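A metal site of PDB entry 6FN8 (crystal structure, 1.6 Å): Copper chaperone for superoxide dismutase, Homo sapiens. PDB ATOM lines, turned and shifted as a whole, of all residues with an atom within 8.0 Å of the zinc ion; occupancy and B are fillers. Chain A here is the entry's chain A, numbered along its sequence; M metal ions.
OD2 of Asp 83 lies within hydrogen-bond range of N of Gly 72, 3.0 Å away.
The backbone carbonyl oxygen (O) of Asp 83 sits close to the guanidinium group (NH2) of Arg 79.
The backbone NH (N) of His 80 sits at hydrogen-bond distance from the backbone carbonyl oxygen (O) of Ser 70.
O of Ala 69 lies close to NE2 of His 80, at 3.3 Å.
O of Thr 134 sits close to NE2 of His 71, 3.5 Å away.
A ring nitrogen (NE2) of His 71 is in hydrogen-bond range of the side-chain carboxylate (OD1) of Asp 121 (2.8 Å).
The backbone NH (N) of His 71 is in hydrogen-bond range of the backbone carbonyl oxygen (O) of Lys 132 (2.9 Å).
A ring nitrogen (NE2) of His 63 lies within hydrogen-bond range of a ring nitrogen (ND1) of His 46.
The zinc ion is bound by OD1 of Asp 83, ND1 of His 80, ND1 of His 71 and ND1 of His 63.
The zinc ion has four donor atoms within binding distance.
Slightly farther from the zinc ion lies OD2 of Asp 83 (2.8 Å).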
ATOM      1  N   LEU A  45     -12.591   5.885  20.968  1.00  0.00           N
ATOM      2  CA  LEU A  45     -11.237   5.574  21.416  1.00  0.00           C
ATOM      3  C   LEU A  45     -10.933   6.415  22.663  1.00  0.00           C
ATOM      4  O   LEU A  45     -11.117   7.630  22.651  1.00  0.00           O
ATOM      5  CB  LEU A  45     -10.230   5.937  20.309  1.00  0.00           C
ATOM      6  CG  LEU A  45      -8.780   5.580  20.651  1.00  0.00           C
ATOM      7  CD1 LEU A  45      -8.577   4.091  20.482  1.00  0.00           C
ATOM      8  CD2 LEU A  45      -7.820   6.373  19.766  1.00  0.00           C
ATOM      9  N   HIS A  46     -10.599   5.751  23.772  1.00  0.00           N
ATOM     10  CA  HIS A  46     -10.366   6.466  25.019  1.00  0.00           C
ATOM     11  C   HIS A  46      -9.193   5.895  25.786  1.00  0.00           C
ATOM     12  O   HIS A  46      -8.942   4.690  25.769  1.00  0.00           O
ATOM     13  CB  HIS A  46     -11.605   6.445  25.914  1.00  0.00           C
ATOM     14  CG  HIS A  46     -12.879   6.689  25.176  1.00  0.00           C
ATOM     15  ND1 HIS A  46     -13.654   5.660  24.689  1.00  0.00           N
ATOM     16  CD2 HIS A  46     -13.461   7.836  24.755  1.00  0.00           C
ATOM     17  CE1 HIS A  46     -14.670   6.165  24.008  1.00  0.00           C
ATOM     18  NE2 HIS A  46     -14.557   7.481  24.006  1.00  0.00           N
ATOM     19  N   VAL A  47      -8.529   6.773  26.540  1.00  0.00           N
ATOM     20  CA  VAL A  47      -7.622   6.322  27.577  1.00  0.00           C
ATOM     21  C   VAL A  47      -8.389   6.145  28.876  1.00  0.00           C
ATOM     22  O   VAL A  47      -9.141   7.034  29.292  1.00  0.00           O
ATOM     23  CB  VAL A  47      -6.475   7.325  27.759  1.00  0.00           C
ATOM     24  CG1 VAL A  47      -5.618   6.931  28.954  1.00  0.00           C
ATOM     25  CG2 VAL A  47      -5.655   7.393  26.477  1.00  0.00           C
ATOM     26  N   HIS A  48      -8.202   4.985  29.510  1.00  0.00           N
ATOM     27  CA  HIS A  48      -8.887   4.661  30.770  1.00  0.00           C
ATOM     28  C   HIS A  48      -7.909   4.760  31.937  1.00  0.00           C
ATOM     29  O   HIS A  48      -6.689   4.825  31.737  1.00  0.00           O
ATOM     30  CB  HIS A  48      -9.497   3.259  30.685  1.00  0.00           C
ATOM     31  CG  HIS A  48     -10.690   3.158  29.783  1.00  0.00           C
ATOM     32  ND1 HIS A  48     -11.923   2.746  30.236  1.00  0.00           N
ATOM     33  CD2 HIS A  48     -10.858   3.511  28.482  1.00  0.00           C
ATOM     34  CE1 HIS A  48     -12.770   2.722  29.215  1.00  0.00           C
ATOM     35  NE2 HIS A  48     -12.170   3.229  28.160  1.00  0.00           N
ATOM     36  N   ASN A  62     -12.595   3.455  34.324  1.00  0.00           N
ATOM     37  CA  ASN A  62     -13.393   4.322  33.447  1.00  0.00           C
ATOM     38  C   ASN A  62     -12.472   5.236  32.630  1.00  0.00           C
ATOM     39  O   ASN A  62     -11.248   5.188  32.786  1.00  0.00           O
ATOM     40  CB  ASN A  62     -14.336   5.167  34.309  1.00  0.00           C
ATOM     41  CG  ASN A  62     -15.345   4.314  35.047  1.00  0.00           C
ATOM     42  OD1 ASN A  62     -15.574   4.509  36.244  1.00  0.00           O
ATOM     43  ND2 ASN A  62     -15.831   3.273  34.393  1.00  0.00           N
ATOM     44  N   HIS A  63     -13.054   6.050  31.741  1.00  0.00           N
ATOM     45  CA  HIS A  63     -12.240   7.040  31.025  1.00  0.00           C
ATOM     46  C   HIS A  63     -11.391   7.826  32.017  1.00  0.00           C
ATOM     47  O   HIS A  63     -11.876   8.272  33.056  1.00  0.00           O
ATOM     48  CB  HIS A  63     -13.116   8.025  30.228  1.00  0.00           C
ATOM     49  CG  HIS A  63     -13.964   7.376  29.179  1.00  0.00           C
ATOM     50  ND1 HIS A  63     -14.899   8.080  28.451  1.00  0.00           N
ATOM     51  CD2 HIS A  63     -14.021   6.105  28.722  1.00  0.00           C
ATOM     52  CE1 HIS A  63     -15.542   7.255  27.648  1.00  0.00           C
ATOM     53  NE2 HIS A  63     -15.023   6.044  27.787  1.00  0.00           N
ATOM     54  N   PHE A  64     -10.123   8.022  31.670  1.00  0.00           N
ATOM     55  CA  PHE A  64      -9.211   8.784  32.518  1.00  0.00           C
ATOM     56  C   PHE A  64      -9.739  10.208  32.720  1.00  0.00           C
ATOM     57  O   PHE A  64     -10.008  10.919  31.749  1.00  0.00           O
ATOM     58  CB  PHE A  64      -7.828   8.792  31.877  1.00  0.00           C
ATOM     59  CG  PHE A  64      -6.785   9.550  32.640  1.00  0.00           C
ATOM     60  CD1 PHE A  64      -6.647   9.384  34.012  1.00  0.00           C
ATOM     61  CD2 PHE A  64      -5.898  10.377  31.978  1.00  0.00           C
ATOM     62  CE1 PHE A  64      -5.706  10.110  34.713  1.00  0.00           C
ATOM     63  CE2 PHE A  64      -4.924  11.077  32.674  1.00  0.00           C
ATOM     64  CZ  PHE A  64      -4.805  10.912  34.034  1.00  0.00           C
ATOM     65  N   ASN A  65      -9.975  10.592  33.978  1.00  0.00           N
ATOM     66  CA  ASN A  65     -10.736  11.812  34.264  1.00  0.00           C
ATOM     67  C   ASN A  65     -10.251  12.566  35.508  1.00  0.00           C
ATOM     68  O   ASN A  65     -11.024  12.795  36.452  1.00  0.00           O
ATOM     69  CB  ASN A  65     -12.233  11.501  34.388  1.00  0.00           C
ATOM     70  CG  ASN A  65     -13.085  12.754  34.522  1.00  0.00           C
ATOM     71  OD1 ASN A  65     -12.745  13.825  34.004  1.00  0.00           O
ATOM     72  ND2 ASN A  65     -14.275  12.579  35.097  1.00  0.00           N
ATOM     73  N   ALA A  69     -14.327  16.060  34.971  1.00  0.00           N
ATOM     74  CA  ALA A  69     -15.140  16.666  33.925  1.00  0.00           C
ATOM     75  C   ALA A  69     -16.234  15.706  33.470  1.00  0.00           C
ATOM     76  O   ALA A  69     -16.245  14.537  33.854  1.00  0.00           O
ATOM     77  CB  ALA A  69     -14.262  17.077  32.742  1.00  0.00           C
ATOM     78  N   SER A  70     -17.141  16.193  32.626  1.00  0.00           N
ATOM     79  CA  SER A  70     -18.062  15.302  31.914  1.00  0.00           C
ATOM     80  C   SER A  70     -17.416  14.747  30.659  1.00  0.00           C
ATOM     81  O   SER A  70     -16.431  15.294  30.162  1.00  0.00           O
ATOM     82  CB  SER A  70     -19.351  16.048  31.540  1.00  0.00           C
ATOM     83  OG  SER A  70     -20.096  16.376  32.693  1.00  0.00           O
ATOM     84  N   HIS A  71     -18.037  13.730  30.085  1.00  0.00           N
ATOM     85  CA  HIS A  71     -17.567  13.174  28.813  1.00  0.00           C
ATOM     86  C   HIS A  71     -17.808  14.150  27.661  1.00  0.00           C
ATOM     87  O   HIS A  71     -18.845  14.813  27.605  1.00  0.00           O
ATOM     88  CB  HIS A  71     -18.277  11.853  28.516  1.00  0.00           C
ATOM     89  CG  HIS A  71     -17.835  11.208  27.242  1.00  0.00           C
ATOM     90  ND1 HIS A  71     -16.656  10.513  27.125  1.00  0.00           N
ATOM     91  CD2 HIS A  71     -18.367  11.268  25.993  1.00  0.00           C
ATOM     92  CE1 HIS A  71     -16.484  10.137  25.867  1.00  0.00           C
ATOM     93  NE2 HIS A  71     -17.524  10.558  25.163  1.00  0.00           N
ATOM     94  N   GLY A  72     -16.819  14.274  26.770  1.00  0.00           N
ATOM     95  CA  GLY A  72     -16.976  15.128  25.596  1.00  0.00           C
ATOM     96  C   GLY A  72     -16.123  14.642  24.443  1.00  0.00           C
ATOM     97  O   GLY A  72     -15.569  13.536  24.492  1.00  0.00           O
ATOM     98  N   GLY A  73     -16.055  15.445  23.384  1.00  0.00           N
ATOM     99  CA  GLY A  73     -15.182  15.170  22.255  1.00  0.00           C
ATOM    100  C   GLY A  73     -13.828  15.843  22.410  1.00  0.00           C
ATOM    101  O   GLY A  73     -13.663  16.678  23.301  1.00  0.00           O
ATOM    102  N   ARG A  79     -14.267  17.888  28.670  1.00  0.00           N
ATOM    103  CA  ARG A  79     -14.028  16.499  28.260  1.00  0.00           C
ATOM    104  C   ARG A  79     -13.211  15.784  29.342  1.00  0.00           C
ATOM    105  O   ARG A  79     -12.462  16.421  30.088  1.00  0.00           O
ATOM    106  CB  ARG A  79     -13.283  16.466  26.924  1.00  0.00           C
ATOM    107  CG  ARG A  79     -11.913  17.141  26.956  1.00  0.00           C
ATOM    108  CD  ARG A  79     -11.048  16.726  25.770  1.00  0.00           C
ATOM    109  NE  ARG A  79      -9.956  15.843  26.158  1.00  0.00           N
ATOM    110  CZ  ARG A  79      -8.992  15.445  25.333  1.00  0.00           C
ATOM    111  NH1 ARG A  79      -8.051  14.618  25.754  1.00  0.00           N
ATOM    112  NH2 ARG A  79      -8.929  15.946  24.100  1.00  0.00           N
ATOM    113  N   HIS A  80     -13.334  14.465  29.417  1.00  0.00           N
ATOM    114  CA  HIS A  80     -12.393  13.665  30.189  1.00  0.00           C
ATOM    115  C   HIS A  80     -11.017  13.776  29.533  1.00  0.00           C
ATOM    116  O   HIS A  80     -10.918  13.836  28.307  1.00  0.00           O
ATOM    117  CB  HIS A  80     -12.804  12.198  30.193  1.00  0.00           C
ATOM    118  CG  HIS A  80     -14.179  11.957  30.749  1.00  0.00           C
ATOM    119  ND1 HIS A  80     -15.022  10.981  30.258  1.00  0.00           N
ATOM    120  CD2 HIS A  80     -14.825  12.526  31.799  1.00  0.00           C
ATOM    121  CE1 HIS A  80     -16.116  10.939  31.002  1.00  0.00           C
ATOM    122  NE2 HIS A  80     -16.005  11.839  31.959  1.00  0.00           N
ATOM    123  N   ARG A  81      -9.968  13.800  30.332  1.00  0.00           N
ATOM    124  CA  ARG A  81      -8.648  13.896  29.710  1.00  0.00           C
ATOM    125  C   ARG A  81      -8.394  12.726  28.762  1.00  0.00           C
ATOM    126  O   ARG A  81      -7.761  12.894  27.727  1.00  0.00           O
ATOM    127  CB  ARG A  81      -7.542  14.019  30.751  1.00  0.00           C
ATOM    128  CG  ARG A  81      -6.320  14.724  30.174  1.00  0.00           C
ATOM    129  CD  ARG A  81      -5.282  14.969  31.237  1.00  0.00           C
ATOM    130  NE  ARG A  81      -5.639  16.070  32.128  1.00  0.00           N
ATOM    131  CZ  ARG A  81      -4.978  16.346  33.240  1.00  0.00           C
ATOM    132  NH1 ARG A  81      -3.977  15.550  33.614  1.00  0.00           N
ATOM    133  NH2 ARG A  81      -5.330  17.359  34.005  1.00  0.00           N
ATOM    134  N   GLY A  82      -9.038  11.590  29.031  1.00  0.00           N
ATOM    135  CA  GLY A  82      -8.876  10.407  28.199  1.00  0.00           C
ATOM    136  C   GLY A  82      -9.723  10.354  26.935  1.00  0.00           C
ATOM    137  O   GLY A  82      -9.713   9.345  26.229  1.00  0.00           O
ATOM    138  N   ASP A  83     -10.514  11.411  26.667  1.00  0.00           N
ATOM    139  CA  ASP A  83     -11.459  11.372  25.556  1.00  0.00           C
ATOM    140  C   ASP A  83     -10.793  11.717  24.228  1.00  0.00           C
ATOM    141  O   ASP A  83     -10.550  12.888  23.940  1.00  0.00           O
ATOM    142  CB  ASP A  83     -12.617  12.351  25.794  1.00  0.00           C
ATOM    143  CG  ASP A  83     -13.574  11.868  26.867  1.00  0.00           C
ATOM    144  OD1 ASP A  83     -13.533  10.677  27.209  1.00  0.00           O
ATOM    145  OD2 ASP A  83     -14.388  12.688  27.337  1.00  0.00           O
ATOM    146  N   LEU A  84     -10.656  10.725  23.352  1.00  0.00           N
ATOM    147  CA  LEU A  84      -9.985  10.948  22.067  1.00  0.00           C
ATOM    148  C   LEU A  84     -10.935  10.869  20.876  1.00  0.00           C
ATOM    149  O   LEU A  84     -10.509  10.899  19.728  1.00  0.00           O
ATOM    150  CB  LEU A  84      -8.847   9.940  21.880  1.00  0.00           C
ATOM    151  CG  LEU A  84      -7.727  10.026  22.910  1.00  0.00           C
ATOM    152  CD1 LEU A  84      -6.717   8.901  22.730  1.00  0.00           C
ATOM    153  CD2 LEU A  84      -7.036  11.390  22.855  1.00  0.00           C
ATOM    154  N   GLY A  85     -12.243  10.859  21.153  1.00  0.00           N
ATOM    155  CA  GLY A  85     -13.239  10.866  20.086  1.00  0.00           C
ATOM    156  C   GLY A  85     -13.292   9.552  19.327  1.00  0.00           C
ATOM    157  O   GLY A  85     -13.169   8.488  19.916  1.00  0.00           O
ATOM    158  N   ASP A 121     -18.670   6.958  19.529  1.00  0.00           N
ATOM    159  CA  ASP A 121     -18.732   7.935  20.623  1.00  0.00           C
ATOM    160  C   ASP A 121     -19.590   9.128  20.156  1.00  0.00           C
ATOM    161  O   ASP A 121     -19.244   9.777  19.151  1.00  0.00           O
ATOM    162  CB  ASP A 121     -17.291   8.408  20.914  1.00  0.00           C
ATOM    163  CG  ASP A 121     -17.168   9.231  22.172  1.00  0.00           C
ATOM    164  OD1 ASP A 121     -18.107   9.973  22.536  1.00  0.00           O
ATOM    165  OD2 ASP A 121     -16.018   9.278  22.705  1.00  0.00           O
ATOM    166  N   GLY A 124     -20.658  13.315  23.756  1.00  0.00           N
ATOM    167  CA  GLY A 124     -21.427  14.010  24.790  1.00  0.00           C
ATOM    168  C   GLY A 124     -22.634  14.768  24.266  1.00  0.00           C
ATOM    169  O   GLY A 124     -23.334  15.419  25.041  1.00  0.00           O
ATOM    170  N   LEU A 130     -26.348   8.096  28.631  1.00  0.00           N
ATOM    171  CA  LEU A 130     -24.919   7.801  28.752  1.00  0.00           C
ATOM    172  C   LEU A 130     -24.048   8.866  28.090  1.00  0.00           C
ATOM    173  O   LEU A 130     -22.819   8.804  28.189  1.00  0.00           O
ATOM    174  CB  LEU A 130     -24.592   6.415  28.190  1.00  0.00           C
ATOM    175  CG  LEU A 130     -25.100   5.235  29.026  1.00  0.00           C
ATOM    176  CD1 LEU A 130     -24.840   3.922  28.297  1.00  0.00           C
ATOM    177  CD2 LEU A 130     -24.475   5.228  30.411  1.00  0.00           C
ATOM    178  N   SER A 131     -24.655   9.839  27.420  1.00  0.00           N
ATOM    179  CA  SER A 131     -23.879  10.739  26.560  1.00  0.00           C
ATOM    180  C   SER A 131     -22.743  11.453  27.297  1.00  0.00           C
ATOM    181  O   SER A 131     -21.615  11.508  26.800  1.00  0.00           O
ATOM    182  CB  SER A 131     -24.782  11.766  25.875  1.00  0.00           C
ATOM    183  OG  SER A 131     -25.607  11.144  24.911  1.00  0.00           O
ATOM    184  N   LYS A 132     -23.049  12.030  28.466  1.00  0.00           N
ATOM    185  CA  LYS A 132     -22.062  12.818  29.194  1.00  0.00           C
ATOM    186  C   LYS A 132     -21.283  11.983  30.196  1.00  0.00           C
ATOM    187  O   LYS A 132     -20.499  12.517  30.988  1.00  0.00           O
ATOM    188  CB  LYS A 132     -22.743  13.987  29.911  1.00  0.00           C
ATOM    189  CG  LYS A 132     -23.439  14.949  28.972  1.00  0.00           C
ATOM    190  CD  LYS A 132     -22.519  16.103  28.610  1.00  0.00           C
ATOM    191  CE  LYS A 132     -23.284  17.186  27.877  1.00  0.00           C
ATOM    192  NZ  LYS A 132     -22.624  17.545  26.593  1.00  0.00           N
ATOM    193  N   ILE A 133     -21.509  10.670  30.175  1.00  0.00           N
ATOM    194  CA  ILE A 133     -20.789   9.755  31.050  1.00  0.00           C
ATOM    195  C   ILE A 133     -19.785   8.902  30.266  1.00  0.00           C
ATOM    196  O   ILE A 133     -18.589   8.927  30.551  1.00  0.00           O
ATOM    197  CB  ILE A 133     -21.771   8.884  31.877  1.00  0.00           C
ATOM    198  CG1 ILE A 133     -22.621   9.784  32.767  1.00  0.00           C
ATOM    199  CG2 ILE A 133     -21.000   7.885  32.727  1.00  0.00           C
ATOM    200  CD1 ILE A 133     -23.894   9.138  33.275  1.00  0.00           C
ATOM    201  N   THR A 134     -20.240   8.265  29.190  1.00  0.00           N
ATOM    202  CA  THR A 134     -19.325   7.444  28.375  1.00  0.00           C
ATOM    203  C   THR A 134     -19.288   7.852  26.898  1.00  0.00           C
ATOM    204  O   THR A 134     -18.448   7.367  26.152  1.00  0.00           O
ATOM    205  CB  THR A 134     -19.688   5.944  28.408  1.00  0.00           C
ATOM    206  OG1 THR A 134     -21.007   5.767  27.871  1.00  0.00           O
ATOM    207  CG2 THR A 134     -19.616   5.385  29.836  1.00  0.00           C
ATOM    208  N   GLY A 135     -20.309   8.575  26.443  1.00  0.00           N
ATOM    209  CA  GLY A 135     -20.498   8.776  25.015  1.00  0.00           C
ATOM    210  C   GLY A 135     -21.316   7.698  24.323  1.00  0.00           C
ATOM    211  O   GLY A 135     -21.517   7.757  23.116  1.00  0.00           O
HETATM  212 ZN    ZN M   1     -15.042  10.147  28.369  1.00  0.00          ZN
